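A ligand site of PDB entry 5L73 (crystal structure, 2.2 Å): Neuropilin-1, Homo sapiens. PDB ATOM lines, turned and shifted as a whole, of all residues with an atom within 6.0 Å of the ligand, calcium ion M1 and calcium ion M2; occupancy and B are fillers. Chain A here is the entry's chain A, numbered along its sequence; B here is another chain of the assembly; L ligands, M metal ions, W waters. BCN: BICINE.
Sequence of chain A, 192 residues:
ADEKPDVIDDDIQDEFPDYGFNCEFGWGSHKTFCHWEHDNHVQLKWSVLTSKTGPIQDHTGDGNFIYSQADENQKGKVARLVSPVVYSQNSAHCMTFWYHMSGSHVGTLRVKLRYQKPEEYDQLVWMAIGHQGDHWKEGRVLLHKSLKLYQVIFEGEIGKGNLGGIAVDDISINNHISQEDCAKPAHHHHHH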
ATOM      1  N   CYS A  23     -21.786  12.778 -27.441  1.00  0.00           N
ATOM      2  CA  CYS A  23     -21.329  13.419 -28.663  1.00  0.00           C
ATOM      3  C   CYS A  23     -21.214  14.933 -28.583  1.00  0.00           C
ATOM      4  O   CYS A  23     -22.181  15.619 -28.273  1.00  0.00           O
ATOM      5  CB  CYS A  23     -22.225  13.051 -29.846  1.00  0.00           C
ATOM      6  SG  CYS A  23     -21.446  13.299 -31.472  1.00  0.00           S
ATOM      7  N   GLU A  24     -20.009  15.429 -28.865  1.00  0.00           N
ATOM      8  CA  GLU A  24     -19.699  16.835 -28.974  1.00  0.00           C
ATOM      9  C   GLU A  24     -19.672  17.307 -30.453  1.00  0.00           C
ATOM     10  O   GLU A  24     -19.486  18.492 -30.711  1.00  0.00           O
ATOM     11  CB  GLU A  24     -18.311  17.107 -28.321  1.00  0.00           C
ATOM     12  CG  GLU A  24     -18.407  17.545 -26.871  1.00  0.00           C
ATOM     13  CD  GLU A  24     -18.886  19.006 -26.728  1.00  0.00           C
ATOM     14  OE1 GLU A  24     -18.778  19.579 -25.630  1.00  0.00           O
ATOM     15  OE2 GLU A  24     -19.361  19.607 -27.704  1.00  0.00           O
ATOM     16  N   PHE A  25     -19.812  16.348 -31.379  1.00  0.00           N
ATOM     17  CA  PHE A  25     -19.825  16.551 -32.838  1.00  0.00           C
ATOM     18  C   PHE A  25     -18.475  16.895 -33.447  1.00  0.00           C
ATOM     19  O   PHE A  25     -18.405  17.430 -34.549  1.00  0.00           O
ATOM     20  CB  PHE A  25     -20.968  17.481 -33.272  1.00  0.00           C
ATOM     21  CG  PHE A  25     -22.298  17.000 -32.789  1.00  0.00           C
ATOM     22  CD1 PHE A  25     -22.918  15.898 -33.384  1.00  0.00           C
ATOM     23  CD2 PHE A  25     -22.892  17.560 -31.665  1.00  0.00           C
ATOM     24  CE1 PHE A  25     -24.142  15.435 -32.923  1.00  0.00           C
ATOM     25  CE2 PHE A  25     -24.108  17.093 -31.184  1.00  0.00           C
ATOM     26  CZ  PHE A  25     -24.730  16.020 -31.809  1.00  0.00           C
ATOM     27  N   GLY A  26     -17.408  16.519 -32.725  1.00  0.00           N
ATOM     28  CA  GLY A  26     -16.051  16.650 -33.144  1.00  0.00           C
ATOM     29  C   GLY A  26     -15.396  17.966 -32.853  1.00  0.00           C
ATOM     30  O   GLY A  26     -15.831  18.717 -31.977  1.00  0.00           O
ATOM     31  N   GLN A  57     -22.211  29.486 -31.589  1.00  0.00           N
ATOM     32  CA  GLN A  57     -20.972  28.753 -31.566  1.00  0.00           C
ATOM     33  C   GLN A  57     -20.816  27.929 -30.294  1.00  0.00           C
ATOM     34  O   GLN A  57     -21.439  28.218 -29.248  1.00  0.00           O
ATOM     35  CB  GLN A  57     -19.773  29.722 -31.684  1.00  0.00           C
ATOM     36  CG  GLN A  57     -19.707  30.569 -32.939  1.00  0.00           C
ATOM     37  CD  GLN A  57     -18.430  31.400 -32.991  1.00  0.00           C
ATOM     38  OE1 GLN A  57     -17.309  30.862 -32.823  1.00  0.00           O
ATOM     39  NE2 GLN A  57     -18.571  32.705 -33.168  1.00  0.00           N
ATOM     40  N   ASP A  58     -19.996  26.897 -30.407  1.00  0.00           N
ATOM     41  CA  ASP A  58     -19.494  26.165 -29.279  1.00  0.00           C
ATOM     42  C   ASP A  58     -18.255  26.940 -28.809  1.00  0.00           C
ATOM     43  O   ASP A  58     -17.129  26.485 -28.984  1.00  0.00           O
ATOM     44  CB  ASP A  58     -19.162  24.729 -29.700  1.00  0.00           C
ATOM     45  CG  ASP A  58     -18.736  23.851 -28.540  1.00  0.00           C
ATOM     46  OD1 ASP A  58     -18.728  24.338 -27.367  1.00  0.00           O
ATOM     47  OD2 ASP A  58     -18.446  22.656 -28.778  1.00  0.00           O
ATOM     48  N   HIS A  59     -18.486  28.117 -28.211  1.00  0.00           N
ATOM     49  CA  HIS A  59     -17.432  29.136 -27.982  1.00  0.00           C
ATOM     50  C   HIS A  59     -16.398  28.610 -27.012  1.00  0.00           C
ATOM     51  O   HIS A  59     -15.220  28.851 -27.160  1.00  0.00           O
ATOM     52  CB  HIS A  59     -17.976  30.430 -27.344  1.00  0.00           C
ATOM     53  CG  HIS A  59     -18.860  31.236 -28.242  1.00  0.00           C
ATOM     54  ND1 HIS A  59     -18.386  32.209 -29.095  1.00  0.00           N
ATOM     55  CD2 HIS A  59     -20.209  31.236 -28.376  1.00  0.00           C
ATOM     56  CE1 HIS A  59     -19.401  32.771 -29.735  1.00  0.00           C
ATOM     57  NE2 HIS A  59     -20.515  32.199 -29.316  1.00  0.00           N
ATOM     58  N   THR A  60     -16.872  27.883 -26.019  1.00  0.00           N
ATOM     59  CA  THR A  60     -16.096  27.531 -24.878  1.00  0.00           C
ATOM     60  C   THR A  60     -15.111  26.392 -25.221  1.00  0.00           C
ATOM     61  O   THR A  60     -14.020  26.354 -24.666  1.00  0.00           O
ATOM     62  CB  THR A  60     -17.050  27.239 -23.696  1.00  0.00           C
ATOM     63  OG1 THR A  60     -17.904  28.396 -23.498  1.00  0.00           O
ATOM     64  CG2 THR A  60     -16.279  26.967 -22.444  1.00  0.00           C
ATOM     65  N   GLY A  61     -15.476  25.501 -26.131  1.00  0.00           N
ATOM     66  CA  GLY A  61     -14.530  24.507 -26.664  1.00  0.00           C
ATOM     67  C   GLY A  61     -13.874  24.822 -28.010  1.00  0.00           C
ATOM     68  O   GLY A  61     -12.998  24.058 -28.434  1.00  0.00           O
ATOM     69  N   GLY A  63     -15.566  24.461 -30.699  1.00  0.00           N
ATOM     70  CA  GLY A  63     -15.907  23.137 -31.177  1.00  0.00           C
ATOM     71  C   GLY A  63     -16.938  23.148 -32.276  1.00  0.00           C
ATOM     72  O   GLY A  63     -17.188  24.175 -32.913  1.00  0.00           O
ATOM     73  N   ASN A  64     -17.510  21.984 -32.513  1.00  0.00           N
ATOM     74  CA  ASN A  64     -18.526  21.822 -33.518  1.00  0.00           C
ATOM     75  C   ASN A  64     -19.866  21.683 -32.833  1.00  0.00           C
ATOM     76  O   ASN A  64     -19.938  21.524 -31.616  1.00  0.00           O
ATOM     77  CB  ASN A  64     -18.227  20.618 -34.398  1.00  0.00           C
ATOM     78  CG  ASN A  64     -16.939  20.773 -35.230  1.00  0.00           C
ATOM     79  OD1 ASN A  64     -16.424  21.891 -35.440  1.00  0.00           O
ATOM     80  ND2 ASN A  64     -16.422  19.640 -35.703  1.00  0.00           N
ATOM     81  N   PHE A  65     -20.932  21.816 -33.622  1.00  0.00           N
ATOM     82  CA  PHE A  65     -22.291  21.565 -33.194  1.00  0.00           C
ATOM     83  C   PHE A  65     -23.152  21.152 -34.387  1.00  0.00           C
ATOM     84  O   PHE A  65     -22.669  21.191 -35.535  1.00  0.00           O
ATOM     85  CB  PHE A  65     -22.858  22.818 -32.492  1.00  0.00           C
ATOM     86  CG  PHE A  65     -22.890  24.043 -33.362  1.00  0.00           C
ATOM     87  CD1 PHE A  65     -21.765  24.859 -33.464  1.00  0.00           C
ATOM     88  CD2 PHE A  65     -24.041  24.384 -34.052  1.00  0.00           C
ATOM     89  CE1 PHE A  65     -21.777  25.964 -34.304  1.00  0.00           C
ATOM     90  CE2 PHE A  65     -24.072  25.503 -34.868  1.00  0.00           C
ATOM     91  CZ  PHE A  65     -22.950  26.305 -34.991  1.00  0.00           C
ATOM     92  N   TRP A  98     -27.405  20.688 -25.052  1.00  0.00           N
ATOM     93  CA  TRP A  98     -27.538  22.099 -25.189  1.00  0.00           C
ATOM     94  C   TRP A  98     -28.235  22.420 -26.485  1.00  0.00           C
ATOM     95  O   TRP A  98     -28.074  21.719 -27.454  1.00  0.00           O
ATOM     96  CB  TRP A  98     -26.164  22.781 -25.150  1.00  0.00           C
ATOM     97  CG  TRP A  98     -25.537  22.683 -23.809  1.00  0.00           C
ATOM     98  CD1 TRP A  98     -24.848  21.601 -23.306  1.00  0.00           C
ATOM     99  CD2 TRP A  98     -25.522  23.677 -22.777  1.00  0.00           C
ATOM    100  NE1 TRP A  98     -24.434  21.860 -22.022  1.00  0.00           N
ATOM    101  CE2 TRP A  98     -24.814  23.123 -21.688  1.00  0.00           C
ATOM    102  CE3 TRP A  98     -26.040  24.963 -22.675  1.00  0.00           C
ATOM    103  CZ2 TRP A  98     -24.605  23.836 -20.487  1.00  0.00           C
ATOM    104  CZ3 TRP A  98     -25.829  25.670 -21.514  1.00  0.00           C
ATOM    105  CH2 TRP A  98     -25.127  25.108 -20.428  1.00  0.00           C
ATOM    106  N   TRP A 136     -27.514  29.827 -25.652  1.00  0.00           N
ATOM    107  CA  TRP A 136     -27.543  28.404 -25.394  1.00  0.00           C
ATOM    108  C   TRP A 136     -28.244  28.088 -24.064  1.00  0.00           C
ATOM    109  O   TRP A 136     -27.967  28.731 -23.028  1.00  0.00           O
ATOM    110  CB  TRP A 136     -26.097  27.877 -25.333  1.00  0.00           C
ATOM    111  CG  TRP A 136     -25.379  27.796 -26.650  1.00  0.00           C
ATOM    112  CD1 TRP A 136     -24.483  28.687 -27.149  1.00  0.00           C
ATOM    113  CD2 TRP A 136     -25.516  26.769 -27.630  1.00  0.00           C
ATOM    114  NE1 TRP A 136     -24.035  28.268 -28.383  1.00  0.00           N
ATOM    115  CE2 TRP A 136     -24.663  27.090 -28.701  1.00  0.00           C
ATOM    116  CE3 TRP A 136     -26.273  25.600 -27.701  1.00  0.00           C
ATOM    117  CZ2 TRP A 136     -24.527  26.280 -29.816  1.00  0.00           C
ATOM    118  CZ3 TRP A 136     -26.152  24.792 -28.824  1.00  0.00           C
ATOM    119  CH2 TRP A 136     -25.262  25.137 -29.864  1.00  0.00           C
ATOM    120  N   ASP A 169     -25.915  20.791 -29.289  1.00  0.00           N
ATOM    121  CA  ASP A 169     -24.559  20.342 -29.017  1.00  0.00           C
ATOM    122  C   ASP A 169     -24.467  19.535 -27.746  1.00  0.00           C
ATOM    123  O   ASP A 169     -25.354  19.549 -26.889  1.00  0.00           O
ATOM    124  CB  ASP A 169     -23.624  21.564 -28.877  1.00  0.00           C
ATOM    125  CG  ASP A 169     -22.140  21.239 -29.128  1.00  0.00           C
ATOM    126  OD1 ASP A 169     -21.836  20.130 -29.591  1.00  0.00           O
ATOM    127  OD2 ASP A 169     -21.256  22.109 -28.862  1.00  0.00           O
ATOM    128  N   ASP A 170     -23.354  18.811 -27.643  1.00  0.00           N
ATOM    129  CA  ASP A 170     -22.890  18.302 -26.381  1.00  0.00           C
ATOM    130  C   ASP A 170     -23.944  17.440 -25.689  1.00  0.00           C
ATOM    131  O   ASP A 170     -24.365  17.724 -24.568  1.00  0.00           O
ATOM    132  CB  ASP A 170     -22.448  19.485 -25.509  1.00  0.00           C
ATOM    133  CG  ASP A 170     -21.696  19.045 -24.262  1.00  0.00           C
ATOM    134  OD1 ASP A 170     -21.346  17.852 -24.154  1.00  0.00           O
ATOM    135  OD2 ASP A 170     -21.452  19.917 -23.412  1.00  0.00           O
ATOM    136  N   THR B  96     -16.274  31.490 -18.098  1.00  0.00           N
ATOM    137  CA  THR B  96     -15.815  30.116 -18.315  1.00  0.00           C
ATOM    138  C   THR B  96     -14.314  30.100 -18.174  1.00  0.00           C
ATOM    139  O   THR B  96     -13.648  31.098 -18.405  1.00  0.00           O
ATOM    140  CB  THR B  96     -16.204  29.554 -19.708  1.00  0.00           C
ATOM    141  OG1 THR B  96     -15.406  30.174 -20.725  1.00  0.00           O
ATOM    142  CG2 THR B  96     -17.695  29.777 -19.997  1.00  0.00           C
ATOM    143  N   GLU B 138     -13.911  21.994 -17.590  1.00  0.00           N
ATOM    144  CA  GLU B 138     -14.535  23.284 -17.834  1.00  0.00           C
ATOM    145  C   GLU B 138     -15.143  23.703 -16.507  1.00  0.00           C
ATOM    146  O   GLU B 138     -15.866  22.937 -15.918  1.00  0.00           O
ATOM    147  CB  GLU B 138     -15.609  23.162 -18.947  1.00  0.00           C
ATOM    148  CG  GLU B 138     -16.475  24.391 -19.287  1.00  0.00           C
ATOM    149  CD  GLU B 138     -17.438  24.183 -20.487  1.00  0.00           C
ATOM    150  OE1 GLU B 138     -18.475  24.923 -20.571  1.00  0.00           O
ATOM    151  OE2 GLU B 138     -17.195  23.305 -21.368  1.00  0.00           O
ATOM    152  N   ARG B 140     -17.421  26.981 -14.694  1.00  0.00           N
ATOM    153  CA  ARG B 140     -18.175  28.184 -15.002  1.00  0.00           C
ATOM    154  C   ARG B 140     -18.753  28.824 -13.771  1.00  0.00           C
ATOM    155  O   ARG B 140     -19.206  28.141 -12.874  1.00  0.00           O
ATOM    156  CB  ARG B 140     -19.346  27.927 -15.940  1.00  0.00           C
ATOM    157  CG  ARG B 140     -19.045  27.418 -17.320  1.00  0.00           C
ATOM    158  CD  ARG B 140     -20.351  27.392 -18.111  1.00  0.00           C
ATOM    159  NE  ARG B 140     -20.445  26.092 -18.720  1.00  0.00           N
ATOM    160  CZ  ARG B 140     -21.343  25.135 -18.488  1.00  0.00           C
ATOM    161  NH1 ARG B 140     -22.388  25.283 -17.684  1.00  0.00           N
ATOM    162  NH2 ARG B 140     -21.187  24.012 -19.145  1.00  0.00           N
ATOM    163  N   ASN B 174     -16.640  35.516 -23.383  1.00  0.00           N
ATOM    164  CA  ASN B 174     -17.082  35.574 -24.798  1.00  0.00           C
ATOM    165  C   ASN B 174     -17.939  34.318 -25.141  1.00  0.00           C
ATOM    166  O   ASN B 174     -17.465  33.348 -25.756  1.00  0.00           O
ATOM    167  CB  ASN B 174     -15.887  35.734 -25.751  1.00  0.00           C
ATOM    168  CG  ASN B 174     -15.378  37.191 -25.870  1.00  0.00           C
ATOM    169  OD1 ASN B 174     -14.717  37.545 -26.870  1.00  0.00           O
ATOM    170  ND2 ASN B 174     -15.666  38.031 -24.872  1.00  0.00           N
ATOM    171  N   ASN B 175     -19.189  34.358 -24.686  1.00  0.00           N
ATOM    172  CA  ASN B 175     -20.168  33.282 -24.905  1.00  0.00           C
ATOM    173  C   ASN B 175     -21.601  33.835 -24.739  1.00  0.00           C
ATOM    174  O   ASN B 175     -21.793  34.942 -24.216  1.00  0.00           O
ATOM    175  CB  ASN B 175     -19.922  32.142 -23.919  1.00  0.00           C
ATOM    176  CG  ASN B 175     -19.983  32.613 -22.480  1.00  0.00           C
ATOM    177  OD1 ASN B 175     -21.051  32.970 -21.995  1.00  0.00           O
ATOM    178  ND2 ASN B 175     -18.859  32.649 -21.801  1.00  0.00           N
ATOM    179  N   HIS B 176     -22.576  33.035 -25.182  1.00  0.00           N
ATOM    180  CA  HIS B 176     -23.993  33.350 -25.035  1.00  0.00           C
ATOM    181  C   HIS B 176     -24.664  32.177 -24.326  1.00  0.00           C
ATOM    182  O   HIS B 176     -25.338  31.366 -24.932  1.00  0.00           O
ATOM    183  CB  HIS B 176     -24.613  33.600 -26.402  1.00  0.00           C
ATOM    184  CG  HIS B 176     -24.000  34.738 -27.146  1.00  0.00           C
ATOM    185  ND1 HIS B 176     -24.249  36.055 -26.839  1.00  0.00           N
ATOM    186  CD2 HIS B 176     -23.141  34.756 -28.191  1.00  0.00           C
ATOM    187  CE1 HIS B 176     -23.581  36.838 -27.658  1.00  0.00           C
ATOM    188  NE2 HIS B 176     -22.901  36.080 -28.492  1.00  0.00           N
ATOM    189  N   ILE B 177     -24.388  32.072 -23.038  1.00  0.00           N
ATOM    190  CA  ILE B 177     -24.860  30.961 -22.199  1.00  0.00           C
ATOM    191  C   ILE B 177     -25.909  31.550 -21.300  1.00  0.00           C
ATOM    192  O   ILE B 177     -25.678  32.571 -20.689  1.00  0.00           O
ATOM    193  CB  ILE B 177     -23.722  30.370 -21.351  1.00  0.00           C
ATOM    194  CG1 ILE B 177     -22.652  29.787 -22.263  1.00  0.00           C
ATOM    195  CG2 ILE B 177     -24.239  29.274 -20.398  1.00  0.00           C
ATOM    196  CD1 ILE B 177     -21.429  29.299 -21.534  1.00  0.00           C
HETATM  197  N1  BCN L   1     -22.034  25.696 -24.735  1.00  0.00           N
HETATM  198  C1  BCN L   1     -21.880  27.038 -25.330  1.00  0.00           C
HETATM  199  C2  BCN L   1     -20.425  27.407 -25.299  1.00  0.00           C
HETATM  200  O21 BCN L   1     -20.159  28.632 -25.130  1.00  0.00           O
HETATM  201  O22 BCN L   1     -19.564  26.512 -25.456  1.00  0.00           O
HETATM  202  C3  BCN L   1     -22.192  25.811 -23.259  1.00  0.00           C
HETATM  203  C4  BCN L   1     -20.933  25.430 -22.531  1.00  0.00           C
HETATM  204  O4  BCN L   1     -20.528  24.121 -22.995  1.00  0.00           O
HETATM  205  C5  BCN L   1     -23.167  24.970 -25.352  1.00  0.00           C
HETATM  206  C6  BCN L   1     -22.869  24.547 -26.796  1.00  0.00           C
HETATM  207  O6  BCN L   1     -21.655  23.795 -26.779  1.00  0.00           O
HETATM  208 CA    CA M   1     -19.448  20.702 -29.634  1.00  0.00          CA
HETATM  209 CA    CA M   2     -19.841  24.270 -25.286  1.00  0.00          CA
HETATM  210  O   HOH W   1     -17.249  20.240 -30.161  1.00  0.00           O
HETATM  211  O   HOH W   2     -17.779  24.038 -24.306  1.00  0.00           O
HETATM  212  O   HOH W   3     -21.882  30.459 -26.192  1.00  0.00           O
HETATM  213  O   HOH W   4     -20.064  22.006 -25.309  1.00  0.00           O
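One residue has an atom within 4 Å of calcium ion M2: Asp 58.
The nearest printed residue that does not touch calcium ion M2 is Thr 60 (4.4 Å).
O21 of the ligand is in hydrogen-bond range of N of Thr 60 (3.5 Å).
The side-chain hydroxyl of Thr 60 lies within hydrogen-bond range of an oxygen (O21) of the ligand (2.8 Å).
The side-chain carboxylate of Glu 138 of chain B lies close to an oxygen (O4) of the ligand, 3.3 Å away.
The backbone NH (N) of His 59 sits close to an oxygen (O22) of the ligand, at 3.4 Å.
Merely in contact with the ligand: Trp 136, Trp 98, Arg 140 of chain B, Asn 175 of chain B and Ile 177 of chain B.
Hydrophobic or aromatic side chains that line the ligand: His 59, Trp 98, Trp 136 and Ile 177 of chain B.
Of the 23 residues printed, 10 come within 4 Å of the ligand.
Water W1 lies within hydrogen-bond range of O of Gly 26 (2.8 Å) and N of Asn 64 (2.9 Å).
Water W2 bridges the side-chain carboxylate (OE2) of Glu 138 of chain B (3.1 Å) and the backbone NH (N) of Gly 61 (3.3 Å).
Water W4 lies within hydrogen-bond range of the side-chain carboxylate of Glu 24 (2.8 Å) and the side-chain carboxylate of Asp 170 (3.1 Å).
Water W3 bridges an oxygen (O21) of the ligand and the backbone NH of His 176 of chain B.
An oxygen (O22) of the ligand is bound to calcium ion M2 (2.3 Å).
Water W4 is bound to calcium ion M2.
Water W2 is bound to calcium ion M2, at 2.3 Å.
The side-chain carboxylate (OD1) of Asp 58 is bound to calcium ion M2.
Calcium ion M2 is bound by O4 of the ligand.
Calcium ion M2 is bound by an oxygen (O6) of the ligand, 2.4 Å away.
Calcium ion M2 is bound by N1 of the ligand (2.7 Å).
Calcium ion M1 is bound by the backbone carbonyl oxygen (O) of Asn 64 (2.2 Å), the side-chain carboxylate (OE2) of Glu 24 (2.2 Å), water W1 (2.3 Å), the side-chain carboxylate (OD2) of Asp 58 (2.4 Å), the side-chain carboxylate (OD2) of Asp 169 (2.4 Å), the side-chain carboxylate (OD1) of Asp 169 (2.5 Å) and the backbone carbonyl oxygen (O) of Glu 24 (2.5 Å).
Calcium ion M1 has seven donor atoms within binding distance.
Within 4 Å of calcium ion M1: Glu 24, Asp 58, Asn 64 and Asp 169.
The nearest printed residue that does not touch calcium ion M1 is Gly 63 (4.4 Å).
The backbone carbonyl oxygen of Phe 25 is in hydrogen-bond range of the side-chain amide nitrogen of Asn 64 (3.2 Å).
N of Gly 63 sits at hydrogen-bond distance from O of Asp 58.
N of Trp 98 sits at hydrogen-bond distance from O of Asp 169 (3.0 Å).
The guanidinium group of Arg 140 of chain B lies within salt-bridge range of the side-chain carboxylate of Glu 138 of chain B, at 2.9 Å.
NE1 of Trp 136 is in hydrogen-bond range of O of Gln 57, 2.7 Å away.
The backbone carbonyl oxygen (O) of His 176 of chain B is in hydrogen-bond range of the backbone NH (N) of Trp 136 (2.8 Å).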
